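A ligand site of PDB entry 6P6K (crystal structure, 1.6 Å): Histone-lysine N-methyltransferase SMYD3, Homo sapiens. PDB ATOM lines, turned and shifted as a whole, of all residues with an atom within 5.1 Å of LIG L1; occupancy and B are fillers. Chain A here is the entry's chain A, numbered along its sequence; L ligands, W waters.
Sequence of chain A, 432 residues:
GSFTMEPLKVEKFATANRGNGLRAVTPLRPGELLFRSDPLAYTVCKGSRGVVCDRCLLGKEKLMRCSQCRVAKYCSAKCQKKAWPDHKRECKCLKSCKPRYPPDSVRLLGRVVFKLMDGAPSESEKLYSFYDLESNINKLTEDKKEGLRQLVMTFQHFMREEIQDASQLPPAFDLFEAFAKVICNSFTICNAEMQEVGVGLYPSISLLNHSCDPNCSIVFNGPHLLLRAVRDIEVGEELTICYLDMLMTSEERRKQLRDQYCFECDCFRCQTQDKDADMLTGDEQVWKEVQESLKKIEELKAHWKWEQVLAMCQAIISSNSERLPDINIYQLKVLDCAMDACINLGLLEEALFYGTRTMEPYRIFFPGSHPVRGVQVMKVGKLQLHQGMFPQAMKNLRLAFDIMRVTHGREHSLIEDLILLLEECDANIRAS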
ATOM      1  N   ASN A  17     -21.391  19.009 -25.914  1.00  0.00           N
ATOM      2  CA  ASN A  17     -22.820  19.172 -25.675  1.00  0.00           C
ATOM      3  C   ASN A  17     -23.356  18.306 -24.541  1.00  0.00           C
ATOM      4  O   ASN A  17     -24.574  18.101 -24.459  1.00  0.00           O
ATOM      5  CB  ASN A  17     -23.620  18.902 -26.968  1.00  0.00           C
ATOM      6  CG  ASN A  17     -23.400  17.501 -27.535  1.00  0.00           C
ATOM      7  OD1 ASN A  17     -23.243  16.521 -26.800  1.00  0.00           O
ATOM      8  ND2 ASN A  17     -23.393  17.407 -28.858  1.00  0.00           N
ATOM      9  N   ARG A  18     -22.488  17.785 -23.664  1.00  0.00           N
ATOM     10  CA  ARG A  18     -22.908  16.938 -22.561  1.00  0.00           C
ATOM     11  C   ARG A  18     -22.400  17.435 -21.222  1.00  0.00           C
ATOM     12  O   ARG A  18     -22.319  16.660 -20.276  1.00  0.00           O
ATOM     13  CB  ARG A  18     -22.419  15.484 -22.751  1.00  0.00           C
ATOM     14  CG  ARG A  18     -22.773  14.839 -24.052  1.00  0.00           C
ATOM     15  CD  ARG A  18     -22.108  13.489 -24.136  1.00  0.00           C
ATOM     16  NE  ARG A  18     -22.609  12.734 -25.284  1.00  0.00           N
ATOM     17  CZ  ARG A  18     -22.110  11.574 -25.690  1.00  0.00           C
ATOM     18  NH1 ARG A  18     -21.094  11.031 -25.034  1.00  0.00           N
ATOM     19  NH2 ARG A  18     -22.622  10.969 -26.741  1.00  0.00           N
ATOM     20  N   GLY A  19     -22.026  18.709 -21.123  1.00  0.00           N
ATOM     21  CA  GLY A  19     -21.483  19.216 -19.879  1.00  0.00           C
ATOM     22  C   GLY A  19     -20.062  18.746 -19.659  1.00  0.00           C
ATOM     23  O   GLY A  19     -19.280  18.578 -20.595  1.00  0.00           O
ATOM     24  N   ASN A  20     -19.709  18.517 -18.395  1.00  0.00           N
ATOM     25  CA  ASN A  20     -18.404  17.936 -18.140  1.00  0.00           C
ATOM     26  C   ASN A  20     -18.457  16.434 -18.381  1.00  0.00           C
ATOM     27  O   ASN A  20     -19.516  15.804 -18.326  1.00  0.00           O
ATOM     28  CB  ASN A  20     -17.944  18.235 -16.728  1.00  0.00           C
ATOM     29  CG  ASN A  20     -17.732  19.705 -16.513  1.00  0.00           C
ATOM     30  OD1 ASN A  20     -17.069  20.361 -17.312  1.00  0.00           O
ATOM     31  ND2 ASN A  20     -18.323  20.247 -15.455  1.00  0.00           N
ATOM     32  N   GLY A  21     -17.288  15.858 -18.655  1.00  0.00           N
ATOM     33  CA  GLY A  21     -17.180  14.436 -18.916  1.00  0.00           C
ATOM     34  C   GLY A  21     -15.832  13.945 -18.436  1.00  0.00           C
ATOM     35  O   GLY A  21     -15.022  14.691 -17.897  1.00  0.00           O
ATOM     36  N   TYR A 128     -13.976  15.754  -8.918  1.00  0.00           N
ATOM     37  CA  TYR A 128     -15.253  16.443  -9.072  1.00  0.00           C
ATOM     38  C   TYR A 128     -15.935  16.372  -7.726  1.00  0.00           C
ATOM     39  O   TYR A 128     -15.942  15.322  -7.084  1.00  0.00           O
ATOM     40  CB  TYR A 128     -16.085  15.761 -10.159  1.00  0.00           C
ATOM     41  CG  TYR A 128     -17.073  16.601 -10.967  1.00  0.00           C
ATOM     42  CD1 TYR A 128     -16.703  17.800 -11.563  1.00  0.00           C
ATOM     43  CD2 TYR A 128     -18.366  16.124 -11.207  1.00  0.00           C
ATOM     44  CE1 TYR A 128     -17.595  18.530 -12.351  1.00  0.00           C
ATOM     45  CE2 TYR A 128     -19.267  16.841 -11.987  1.00  0.00           C
ATOM     46  CZ  TYR A 128     -18.873  18.046 -12.548  1.00  0.00           C
ATOM     47  OH  TYR A 128     -19.776  18.732 -13.330  1.00  0.00           O
ATOM     48  N   ASP A 132     -19.601  20.755  -7.387  1.00  0.00           N
ATOM     49  CA  ASP A 132     -19.447  20.842  -8.839  1.00  0.00           C
ATOM     50  C   ASP A 132     -20.576  20.165  -9.610  1.00  0.00           C
ATOM     51  O   ASP A 132     -20.721  20.444 -10.817  1.00  0.00           O
ATOM     52  CB  ASP A 132     -18.156  20.154  -9.292  1.00  0.00           C
ATOM     53  CG  ASP A 132     -16.892  20.837  -8.813  1.00  0.00           C
ATOM     54  OD1 ASP A 132     -16.893  22.080  -8.675  1.00  0.00           O
ATOM     55  OD2 ASP A 132     -15.889  20.122  -8.614  1.00  0.00           O
ATOM     56  N   LEU A 133     -21.353  19.278  -8.974  1.00  0.00           N
ATOM     57  CA  LEU A 133     -22.261  18.387  -9.699  1.00  0.00           C
ATOM     58  C   LEU A 133     -23.298  19.164 -10.499  1.00  0.00           C
ATOM     59  O   LEU A 133     -23.744  20.254 -10.118  1.00  0.00           O
ATOM     60  CB  LEU A 133     -22.997  17.443  -8.745  1.00  0.00           C
ATOM     61  CG  LEU A 133     -22.121  16.483  -7.961  1.00  0.00           C
ATOM     62  CD1 LEU A 133     -22.995  15.681  -7.012  1.00  0.00           C
ATOM     63  CD2 LEU A 133     -21.356  15.560  -8.899  1.00  0.00           C
ATOM     64  N   GLU A 134     -23.652  18.578 -11.644  1.00  0.00           N
ATOM     65  CA  GLU A 134     -24.733  19.087 -12.476  1.00  0.00           C
ATOM     66  C   GLU A 134     -26.060  19.052 -11.723  1.00  0.00           C
ATOM     67  O   GLU A 134     -26.416  18.041 -11.105  1.00  0.00           O
ATOM     68  CB  GLU A 134     -24.837  18.255 -13.756  1.00  0.00           C
ATOM     69  CG  GLU A 134     -26.047  18.661 -14.604  1.00  0.00           C
ATOM     70  CD  GLU A 134     -25.835  19.987 -15.249  1.00  0.00           C
ATOM     71  OE1 GLU A 134     -25.014  20.046 -16.186  1.00  0.00           O
ATOM     72  OE2 GLU A 134     -26.457  20.993 -14.821  1.00  0.00           O
ATOM     73  N   ASN A 136     -29.002  20.560 -13.427  1.00  0.00           N
ATOM     74  CA  ASN A 136     -30.034  20.631 -14.467  1.00  0.00           C
ATOM     75  C   ASN A 136     -31.198  21.515 -14.054  1.00  0.00           C
ATOM     76  O   ASN A 136     -32.324  21.329 -14.514  1.00  0.00           O
ATOM     77  CB  ASN A 136     -30.551  19.254 -14.859  1.00  0.00           C
ATOM     78  CG  ASN A 136     -29.588  18.523 -15.754  1.00  0.00           C
ATOM     79  OD1 ASN A 136     -29.106  19.096 -16.720  1.00  0.00           O
ATOM     80  ND2 ASN A 136     -29.267  17.279 -15.403  1.00  0.00           N
ATOM     81  N   CYS A 184     -29.961  13.564 -10.398  1.00  0.00           N
ATOM     82  CA  CYS A 184     -29.244  13.168 -11.600  1.00  0.00           C
ATOM     83  C   CYS A 184     -27.824  12.698 -11.319  1.00  0.00           C
ATOM     84  O   CYS A 184     -27.020  12.607 -12.247  1.00  0.00           O
ATOM     85  CB  CYS A 184     -29.254  14.312 -12.626  1.00  0.00           C
ATOM     86  SG  CYS A 184     -28.462  15.868 -12.148  1.00  0.00           S
ATOM     87  N   ASN A 185     -27.514  12.386 -10.056  1.00  0.00           N
ATOM     88  CA  ASN A 185     -26.181  11.893  -9.720  1.00  0.00           C
ATOM     89  C   ASN A 185     -26.198  10.723  -8.741  1.00  0.00           C
ATOM     90  O   ASN A 185     -25.168  10.421  -8.140  1.00  0.00           O
ATOM     91  CB  ASN A 185     -25.335  13.029  -9.154  1.00  0.00           C
ATOM     92  CG  ASN A 185     -24.926  14.017 -10.211  1.00  0.00           C
ATOM     93  OD1 ASN A 185     -24.003  13.759 -10.996  1.00  0.00           O
ATOM     94  ND2 ASN A 185     -25.608  15.179 -10.241  1.00  0.00           N
ATOM     95  N   SER A 206     -19.317  10.732 -10.983  1.00  0.00           N
ATOM     96  CA  SER A 206     -20.387  11.478 -11.617  1.00  0.00           C
ATOM     97  C   SER A 206     -19.945  12.210 -12.865  1.00  0.00           C
ATOM     98  O   SER A 206     -20.796  12.753 -13.565  1.00  0.00           O
ATOM     99  CB  SER A 206     -20.975  12.495 -10.634  1.00  0.00           C
ATOM    100  OG  SER A 206     -22.073  11.940  -9.932  1.00  0.00           O
ATOM    101  N   LEU A 207     -18.647  12.283 -13.154  1.00  0.00           N
ATOM    102  CA  LEU A 207     -18.239  12.904 -14.413  1.00  0.00           C
ATOM    103  C   LEU A 207     -18.628  12.084 -15.628  1.00  0.00           C
ATOM    104  O   LEU A 207     -18.753  12.634 -16.725  1.00  0.00           O
ATOM    105  CB  LEU A 207     -16.730  13.158 -14.434  1.00  0.00           C
ATOM    106  CG  LEU A 207     -16.186  14.383 -13.700  1.00  0.00           C
ATOM    107  CD1 LEU A 207     -14.660  14.331 -13.583  1.00  0.00           C
ATOM    108  CD2 LEU A 207     -16.657  15.657 -14.421  1.00  0.00           C
ATOM    109  N   LEU A 208     -18.855  10.781 -15.461  1.00  0.00           N
ATOM    110  CA  LEU A 208     -19.090   9.915 -16.602  1.00  0.00           C
ATOM    111  C   LEU A 208     -20.470  10.183 -17.191  1.00  0.00           C
ATOM    112  O   LEU A 208     -21.478  10.113 -16.478  1.00  0.00           O
ATOM    113  CB  LEU A 208     -18.984   8.443 -16.196  1.00  0.00           C
ATOM    114  CG  LEU A 208     -17.600   7.982 -15.779  1.00  0.00           C
ATOM    115  CD1 LEU A 208     -17.721   6.818 -14.816  1.00  0.00           C
ATOM    116  CD2 LEU A 208     -16.835   7.526 -16.996  1.00  0.00           C
ATOM    117  N   ASN A 209     -20.505  10.501 -18.479  1.00  0.00           N
ATOM    118  CA  ASN A 209     -21.778  10.611 -19.160  1.00  0.00           C
ATOM    119  C   ASN A 209     -22.293   9.245 -19.572  1.00  0.00           C
ATOM    120  O   ASN A 209     -21.585   8.234 -19.540  1.00  0.00           O
ATOM    121  CB  ASN A 209     -21.641  11.566 -20.345  1.00  0.00           C
ATOM    122  CG  ASN A 209     -21.564  12.989 -19.891  1.00  0.00           C
ATOM    123  OD1 ASN A 209     -22.372  13.429 -19.057  1.00  0.00           O
ATOM    124  ND2 ASN A 209     -20.559  13.724 -20.376  1.00  0.00           N
ATOM    125  N   HIS A 210     -23.572   9.216 -19.917  1.00  0.00           N
ATOM    126  CA  HIS A 210     -24.304   8.001 -20.195  1.00  0.00           C
ATOM    127  C   HIS A 210     -24.152   7.574 -21.644  1.00  0.00           C
ATOM    128  O   HIS A 210     -24.140   8.412 -22.551  1.00  0.00           O
ATOM    129  CB  HIS A 210     -25.784   8.203 -19.901  1.00  0.00           C
ATOM    130  CG  HIS A 210     -26.654   7.144 -20.497  1.00  0.00           C
ATOM    131  ND1 HIS A 210     -26.917   5.950 -19.863  1.00  0.00           N
ATOM    132  CD2 HIS A 210     -27.282   7.089 -21.700  1.00  0.00           C
ATOM    133  CE1 HIS A 210     -27.685   5.207 -20.639  1.00  0.00           C
ATOM    134  NE2 HIS A 210     -27.918   5.875 -21.758  1.00  0.00           N
ATOM    135  N   SER A 211     -24.098   6.262 -21.868  1.00  0.00           N
ATOM    136  CA  SER A 211     -24.320   5.690 -23.183  1.00  0.00           C
ATOM    137  C   SER A 211     -25.122   4.401 -23.030  1.00  0.00           C
ATOM    138  O   SER A 211     -24.925   3.655 -22.073  1.00  0.00           O
ATOM    139  CB  SER A 211     -23.008   5.371 -23.907  1.00  0.00           C
ATOM    140  OG  SER A 211     -23.272   4.674 -25.115  1.00  0.00           O
ATOM    141  N   TYR A 243     -26.247   4.332 -17.505  1.00  0.00           N
ATOM    142  CA  TYR A 243     -26.912   4.647 -16.248  1.00  0.00           C
ATOM    143  C   TYR A 243     -28.038   3.689 -15.897  1.00  0.00           C
ATOM    144  O   TYR A 243     -28.523   3.730 -14.757  1.00  0.00           O
ATOM    145  CB  TYR A 243     -27.534   6.040 -16.286  1.00  0.00           C
ATOM    146  CG  TYR A 243     -26.596   7.207 -16.394  1.00  0.00           C
ATOM    147  CD1 TYR A 243     -25.210   7.040 -16.387  1.00  0.00           C
ATOM    148  CD2 TYR A 243     -27.102   8.495 -16.469  1.00  0.00           C
ATOM    149  CE1 TYR A 243     -24.355   8.146 -16.470  1.00  0.00           C
ATOM    150  CE2 TYR A 243     -26.276   9.593 -16.558  1.00  0.00           C
ATOM    151  CZ  TYR A 243     -24.906   9.423 -16.574  1.00  0.00           C
ATOM    152  OH  TYR A 243     -24.080  10.521 -16.663  1.00  0.00           O
ATOM    153  N   GLN A 260     -35.250  11.657 -15.048  1.00  0.00           N
ATOM    154  CA  GLN A 260     -34.230  11.686 -14.015  1.00  0.00           C
ATOM    155  C   GLN A 260     -33.037  12.538 -14.422  1.00  0.00           C
ATOM    156  O   GLN A 260     -32.474  13.261 -13.580  1.00  0.00           O
ATOM    157  CB  GLN A 260     -33.799  10.243 -13.717  1.00  0.00           C
ATOM    158  CG  GLN A 260     -33.214  10.007 -12.344  1.00  0.00           C
ATOM    159  CD  GLN A 260     -33.104   8.527 -12.009  1.00  0.00           C
ATOM    160  OE1 GLN A 260     -33.555   7.676 -12.779  1.00  0.00           O
ATOM    161  NE2 GLN A 260     -32.490   8.219 -10.879  1.00  0.00           N
ATOM    162  N   TYR A 261     -32.669  12.521 -15.702  1.00  0.00           N
ATOM    163  CA  TYR A 261     -31.385  13.087 -16.119  1.00  0.00           C
ATOM    164  C   TYR A 261     -31.519  14.261 -17.073  1.00  0.00           C
ATOM    165  O   TYR A 261     -30.488  14.847 -17.440  1.00  0.00           O
ATOM    166  CB  TYR A 261     -30.499  12.004 -16.751  1.00  0.00           C
ATOM    167  CG  TYR A 261     -30.163  10.940 -15.728  1.00  0.00           C
ATOM    168  CD1 TYR A 261     -29.278  11.224 -14.693  1.00  0.00           C
ATOM    169  CD2 TYR A 261     -30.751   9.686 -15.770  1.00  0.00           C
ATOM    170  CE1 TYR A 261     -28.962  10.280 -13.727  1.00  0.00           C
ATOM    171  CE2 TYR A 261     -30.440   8.719 -14.796  1.00  0.00           C
ATOM    172  CZ  TYR A 261     -29.544   9.027 -13.799  1.00  0.00           C
ATOM    173  OH  TYR A 261     -29.234   8.102 -12.823  1.00  0.00           O
ATOM    174  N   CYS A 262     -32.736  14.649 -17.446  1.00  0.00           N
ATOM    175  CA  CYS A 262     -32.952  15.802 -18.324  1.00  0.00           C
ATOM    176  C   CYS A 262     -32.067  15.777 -19.569  1.00  0.00           C
ATOM    177  O   CYS A 262     -31.436  16.789 -19.908  1.00  0.00           O
ATOM    178  CB  CYS A 262     -32.726  17.123 -17.576  1.00  0.00           C
ATOM    179  SG  CYS A 262     -33.833  17.422 -16.221  1.00  0.00           S
ATOM    180  N   PHE A 263     -32.013  14.646 -20.270  1.00  0.00           N
ATOM    181  CA  PHE A 263     -31.433  14.703 -21.613  1.00  0.00           C
ATOM    182  C   PHE A 263     -32.114  13.725 -22.559  1.00  0.00           C
ATOM    183  O   PHE A 263     -32.811  12.798 -22.135  1.00  0.00           O
ATOM    184  CB  PHE A 263     -29.911  14.508 -21.626  1.00  0.00           C
ATOM    185  CG  PHE A 263     -29.454  13.102 -21.351  1.00  0.00           C
ATOM    186  CD1 PHE A 263     -29.200  12.694 -20.052  1.00  0.00           C
ATOM    187  CD2 PHE A 263     -29.244  12.220 -22.389  1.00  0.00           C
ATOM    188  CE1 PHE A 263     -28.761  11.418 -19.794  1.00  0.00           C
ATOM    189  CE2 PHE A 263     -28.807  10.913 -22.133  1.00  0.00           C
ATOM    190  CZ  PHE A 263     -28.570  10.532 -20.835  1.00  0.00           C
ATOM    191  N   GLU A 264     -31.918  13.996 -23.852  1.00  0.00           N
ATOM    192  CA  GLU A 264     -32.413  13.190 -24.962  1.00  0.00           C
ATOM    193  C   GLU A 264     -31.231  12.426 -25.518  1.00  0.00           C
ATOM    194  O   GLU A 264     -30.191  13.013 -25.822  1.00  0.00           O
ATOM    195  CB  GLU A 264     -33.020  14.086 -26.049  1.00  0.00           C
ATOM    196  CG  GLU A 264     -33.851  15.287 -25.533  1.00  0.00           C
ATOM    197  CD  GLU A 264     -35.120  14.845 -24.843  1.00  0.00           C
ATOM    198  OE1 GLU A 264     -35.760  15.689 -24.214  1.00  0.00           O
ATOM    199  OE2 GLU A 264     -35.457  13.642 -24.953  1.00  0.00           O
HETATM  200  N1  LIG L   1     -22.223  15.939 -17.731  1.00  0.00           N
HETATM  201  C1  LIG L   1     -22.333  15.770 -16.296  1.00  0.00           C
HETATM  202  C2  LIG L   1     -21.732  16.998 -15.593  1.00  0.00           C
HETATM  203  O1  LIG L   1     -21.553  17.005 -14.376  1.00  0.00           O
HETATM  204  O2  LIG L   1     -21.436  17.996 -16.262  1.00  0.00           O
HETATM  205  C3  LIG L   1     -21.666  14.465 -15.870  1.00  0.00           C
HETATM  206  C4  LIG L   1     -22.652  13.298 -15.842  1.00  0.00           C
HETATM  207  S1  LIG L   1     -23.902  13.532 -14.534  1.00  0.00           S
HETATM  208  C5  LIG L   1     -23.833  11.972 -13.632  1.00  0.00           C
HETATM  209  C6  LIG L   1     -25.478  13.251 -15.388  1.00  0.00           C
HETATM  210  C7  LIG L   1     -25.863  14.425 -16.282  1.00  0.00           C
HETATM  211  O3  LIG L   1     -24.987  14.509 -17.391  1.00  0.00           O
HETATM  212  C8  LIG L   1     -27.235  14.253 -16.904  1.00  0.00           C
HETATM  213  O4  LIG L   1     -28.247  14.623 -16.006  1.00  0.00           O
HETATM  214  C9  LIG L   1     -27.157  15.112 -18.154  1.00  0.00           C
HETATM  215  O5  LIG L   1     -27.253  16.473 -17.762  1.00  0.00           O
HETATM  216  C10 LIG L   1     -25.719  14.861 -18.559  1.00  0.00           C
HETATM  217  N2  LIG L   1     -25.583  13.723 -19.481  1.00  0.00           N
HETATM  218  C11 LIG L   1     -25.157  12.453 -19.153  1.00  0.00           C
HETATM  219  N3  LIG L   1     -25.128  11.682 -20.266  1.00  0.00           N
HETATM  220  C12 LIG L   1     -25.522  12.444 -21.315  1.00  0.00           C
HETATM  221  C13 LIG L   1     -25.674  12.168 -22.664  1.00  0.00           C
HETATM  222  N4  LIG L   1     -25.428  10.969 -23.185  1.00  0.00           N
HETATM  223  N5  LIG L   1     -26.115  13.173 -23.485  1.00  0.00           N
HETATM  224  C14 LIG L   1     -26.380  14.419 -22.985  1.00  0.00           C
HETATM  225  N6  LIG L   1     -26.236  14.694 -21.648  1.00  0.00           N
HETATM  226  C15 LIG L   1     -25.804  13.728 -20.826  1.00  0.00           C
HETATM  227  C1  LG2 L   2     -27.441   0.727 -13.653  1.00  0.00           C
HETATM  228  C2  LG2 L   2     -26.957   1.331 -12.322  1.00  0.00           C
HETATM  229  C3  LG2 L   2     -25.989   0.435 -11.561  1.00  0.00           C
HETATM  230  C4  LG2 L   2     -28.152  -0.583 -13.333  1.00  0.00           C
HETATM  231  C5  LG2 L   2     -26.784  -0.843 -11.284  1.00  0.00           C
HETATM  232  C6  LG2 L   2     -26.427   3.617 -11.889  1.00  0.00           C
HETATM  233  C7  LG2 L   2     -25.700   4.788 -12.346  1.00  0.00           C
HETATM  234  C8  LG2 L   2     -25.934   6.199 -12.004  1.00  0.00           C
HETATM  235  C9  LG2 L   2     -25.003   6.877 -12.697  1.00  0.00           C
HETATM  236  C10 LG2 L   2     -24.746   8.340 -12.728  1.00  0.00           C
HETATM  237  C11 LG2 L   2     -24.862   9.088 -11.449  1.00  0.00           C
HETATM  238  C12 LG2 L   2     -25.893   9.252 -12.504  1.00  0.00           C
HETATM  239  N1  LG2 L   2     -26.274   2.563 -12.671  1.00  0.00           N
HETATM  240  N2  LG2 L   2     -24.706   4.712 -13.190  1.00  0.00           N
HETATM  241  O1  LG2 L   2     -27.087   3.596 -10.852  1.00  0.00           O
HETATM  242  O2  LG2 L   2     -24.241   5.992 -13.431  1.00  0.00           O
HETATM  243  C13 LG2 L   2     -29.038  -4.023 -11.613  1.00  0.00           C
HETATM  244  C14 LG2 L   2     -27.529  -4.199 -11.759  1.00  0.00           C
HETATM  245  N3  LG2 L   2     -29.585  -5.185 -10.893  1.00  0.00           N
HETATM  246  N4  LG2 L   2     -27.330  -1.444 -12.502  1.00  0.00           N
HETATM  247  O3  LG2 L   2     -25.505  -3.132 -13.133  1.00  0.00           O
HETATM  248  O4  LG2 L   2     -27.549  -3.285 -14.291  1.00  0.00           O
HETATM  249  S1  LG2 L   2     -26.934  -3.049 -13.020  1.00  0.00           S
HETATM  250  O   HOH W   1     -27.377  12.960 -26.019  1.00  0.00           O
HETATM  251  O   HOH W   2     -21.774   9.162 -13.817  1.00  0.00           O
HETATM  252  O   HOH W   3     -26.353  16.276 -25.947  1.00  0.00           O
HETATM  253  O   HOH W   4     -24.382  17.856 -17.995  1.00  0.00           O
HETATM  254  O   HOH W   5     -26.046  10.000 -25.958  1.00  0.00           O
HETATM  255  O   HOH W   6     -29.124  17.655 -19.409  1.00  0.00           O
HETATM  256  O   HOH W   7     -27.131  17.335 -21.492  1.00  0.00           O
HETATM  257  O   HOH W   8     -22.192  20.509 -15.542  1.00  0.00           O
HETATM  258  O   HOH W   9     -22.749  15.953 -12.103  1.00  0.00           O
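The side-chain amide oxygen (OD1) of Asn 185 sits close to a sulfur (S1) of LIG L1 (3.5 Å). The backbone carbonyl oxygen (O) of Ser 206 lies close to a sulfur (S1) of LIG L1 (3.3 Å). The side-chain hydroxyl (OH) of Tyr 243 lies close to a sulfur (S1) of LIG L1 (3.7 Å). Gly 19 touches LIG L1 (C to O2, 3.7 Å). CB of Glu 134 touches O1 of LIG L1, at 3.6 Å. Cys 184 touches LIG L1. Leu 207 touches LIG L1 (O to C3, 3.5 Å). O of Leu 208 touches C4 of LIG L1 (3.5 Å). Phe 263 touches LIG L1 (CE2 to C13, 3.4 Å). Within 4 Å of LIG L1: Arg 18, Gly 19, Asn 20, Tyr 128, Glu 134, Asn 136, Cys 184, Asn 185, Ser 206, Leu 207, Leu 208, Asn 209, His 210, Tyr 243, Tyr 261 and Phe 263.
The backbone carbonyl oxygen (O) of Glu 134 sits at hydrogen-bond distance from the side-chain amide nitrogen (ND2) of Asn 185 (3.1 Å). ND1 of His 210 is in hydrogen-bond range of N of Tyr 243 (2.9 Å). OE2 of Glu 134 sits at hydrogen-bond distance from N of Asn 136 (2.9 Å). The backbone carbonyl oxygen (O) of Arg 18 lies within hydrogen-bond range of the side-chain amide nitrogen (ND2) of Asn 209 (3.4 Å). The side-chain hydroxyl (OH) of Tyr 128 is in hydrogen-bond range of the side-chain amide nitrogen (ND2) of Asn 20 (3.0 Å). The side-chain hydroxyl (OH) of Tyr 243 lies within hydrogen-bond range of the backbone carbonyl oxygen (O) of Leu 208, 2.6 Å away. SG of Cys 184 sits at hydrogen-bond distance from ND2 of Asn 136 (3.6 Å). OH of Tyr 128 sits at hydrogen-bond distance from O of Asp 132, 3.2 Å away.
The backbone carbonyl oxygen (O) of Asn 20 is in hydrogen-bond range of a nitrogen (N1) of LIG L1. N1 of LIG L1 sits at hydrogen-bond distance from OD1 of Asn 209 (2.8 Å). N3 of LIG L1 lies within hydrogen-bond range of N of His 210, 2.9 Å away. The backbone carbonyl oxygen (O) of Tyr 243 lies within hydrogen-bond range of a nitrogen (N1) of LG2 L2 (3.3 Å). O of Tyr 261 is in hydrogen-bond range of O4 of LIG L1. O of Arg 18 lies within hydrogen-bond range of N1 of LIG L1, at 2.6 Å. An oxygen (O2) of LIG L1 lies within hydrogen-bond range of the backbone NH (N) of Asn 20, 2.8 Å away. An oxygen (O4) of LIG L1 lies within hydrogen-bond range of the side-chain amide nitrogen (ND2) of Asn 136 (2.9 Å). The backbone carbonyl oxygen of His 210 is in hydrogen-bond range of a nitrogen (N4) of LIG L1. OH of Tyr 128 is in hydrogen-bond range of O1 of LIG L1 (2.7 Å).
Water W8 lies within hydrogen-bond range of an oxygen (O2) of LIG L1 (2.7 Å) and the side-chain carboxylate of Glu 134 (2.9 Å). Water W6 lies within hydrogen-bond range of the backbone carbonyl oxygen (O) of Cys 262, an oxygen (O5) of LIG L1 and the side-chain amide oxygen (OD1) of Asn 136. Water W9 lies within hydrogen-bond range of OD1 of Asn 185 (2.8 Å), O1 of LIG L1 (2.8 Å) and N of Glu 134 (2.8 Å). Water W1 bridges O of Glu 264 and N5 of LIG L1. Water W4 lies within hydrogen-bond range of a nitrogen (N1) of LIG L1 (2.9 Å), the side-chain carboxylate (OE1) of Glu 134 (2.9 Å) and the backbone carbonyl oxygen (O) of Arg 18 (3.3 Å).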
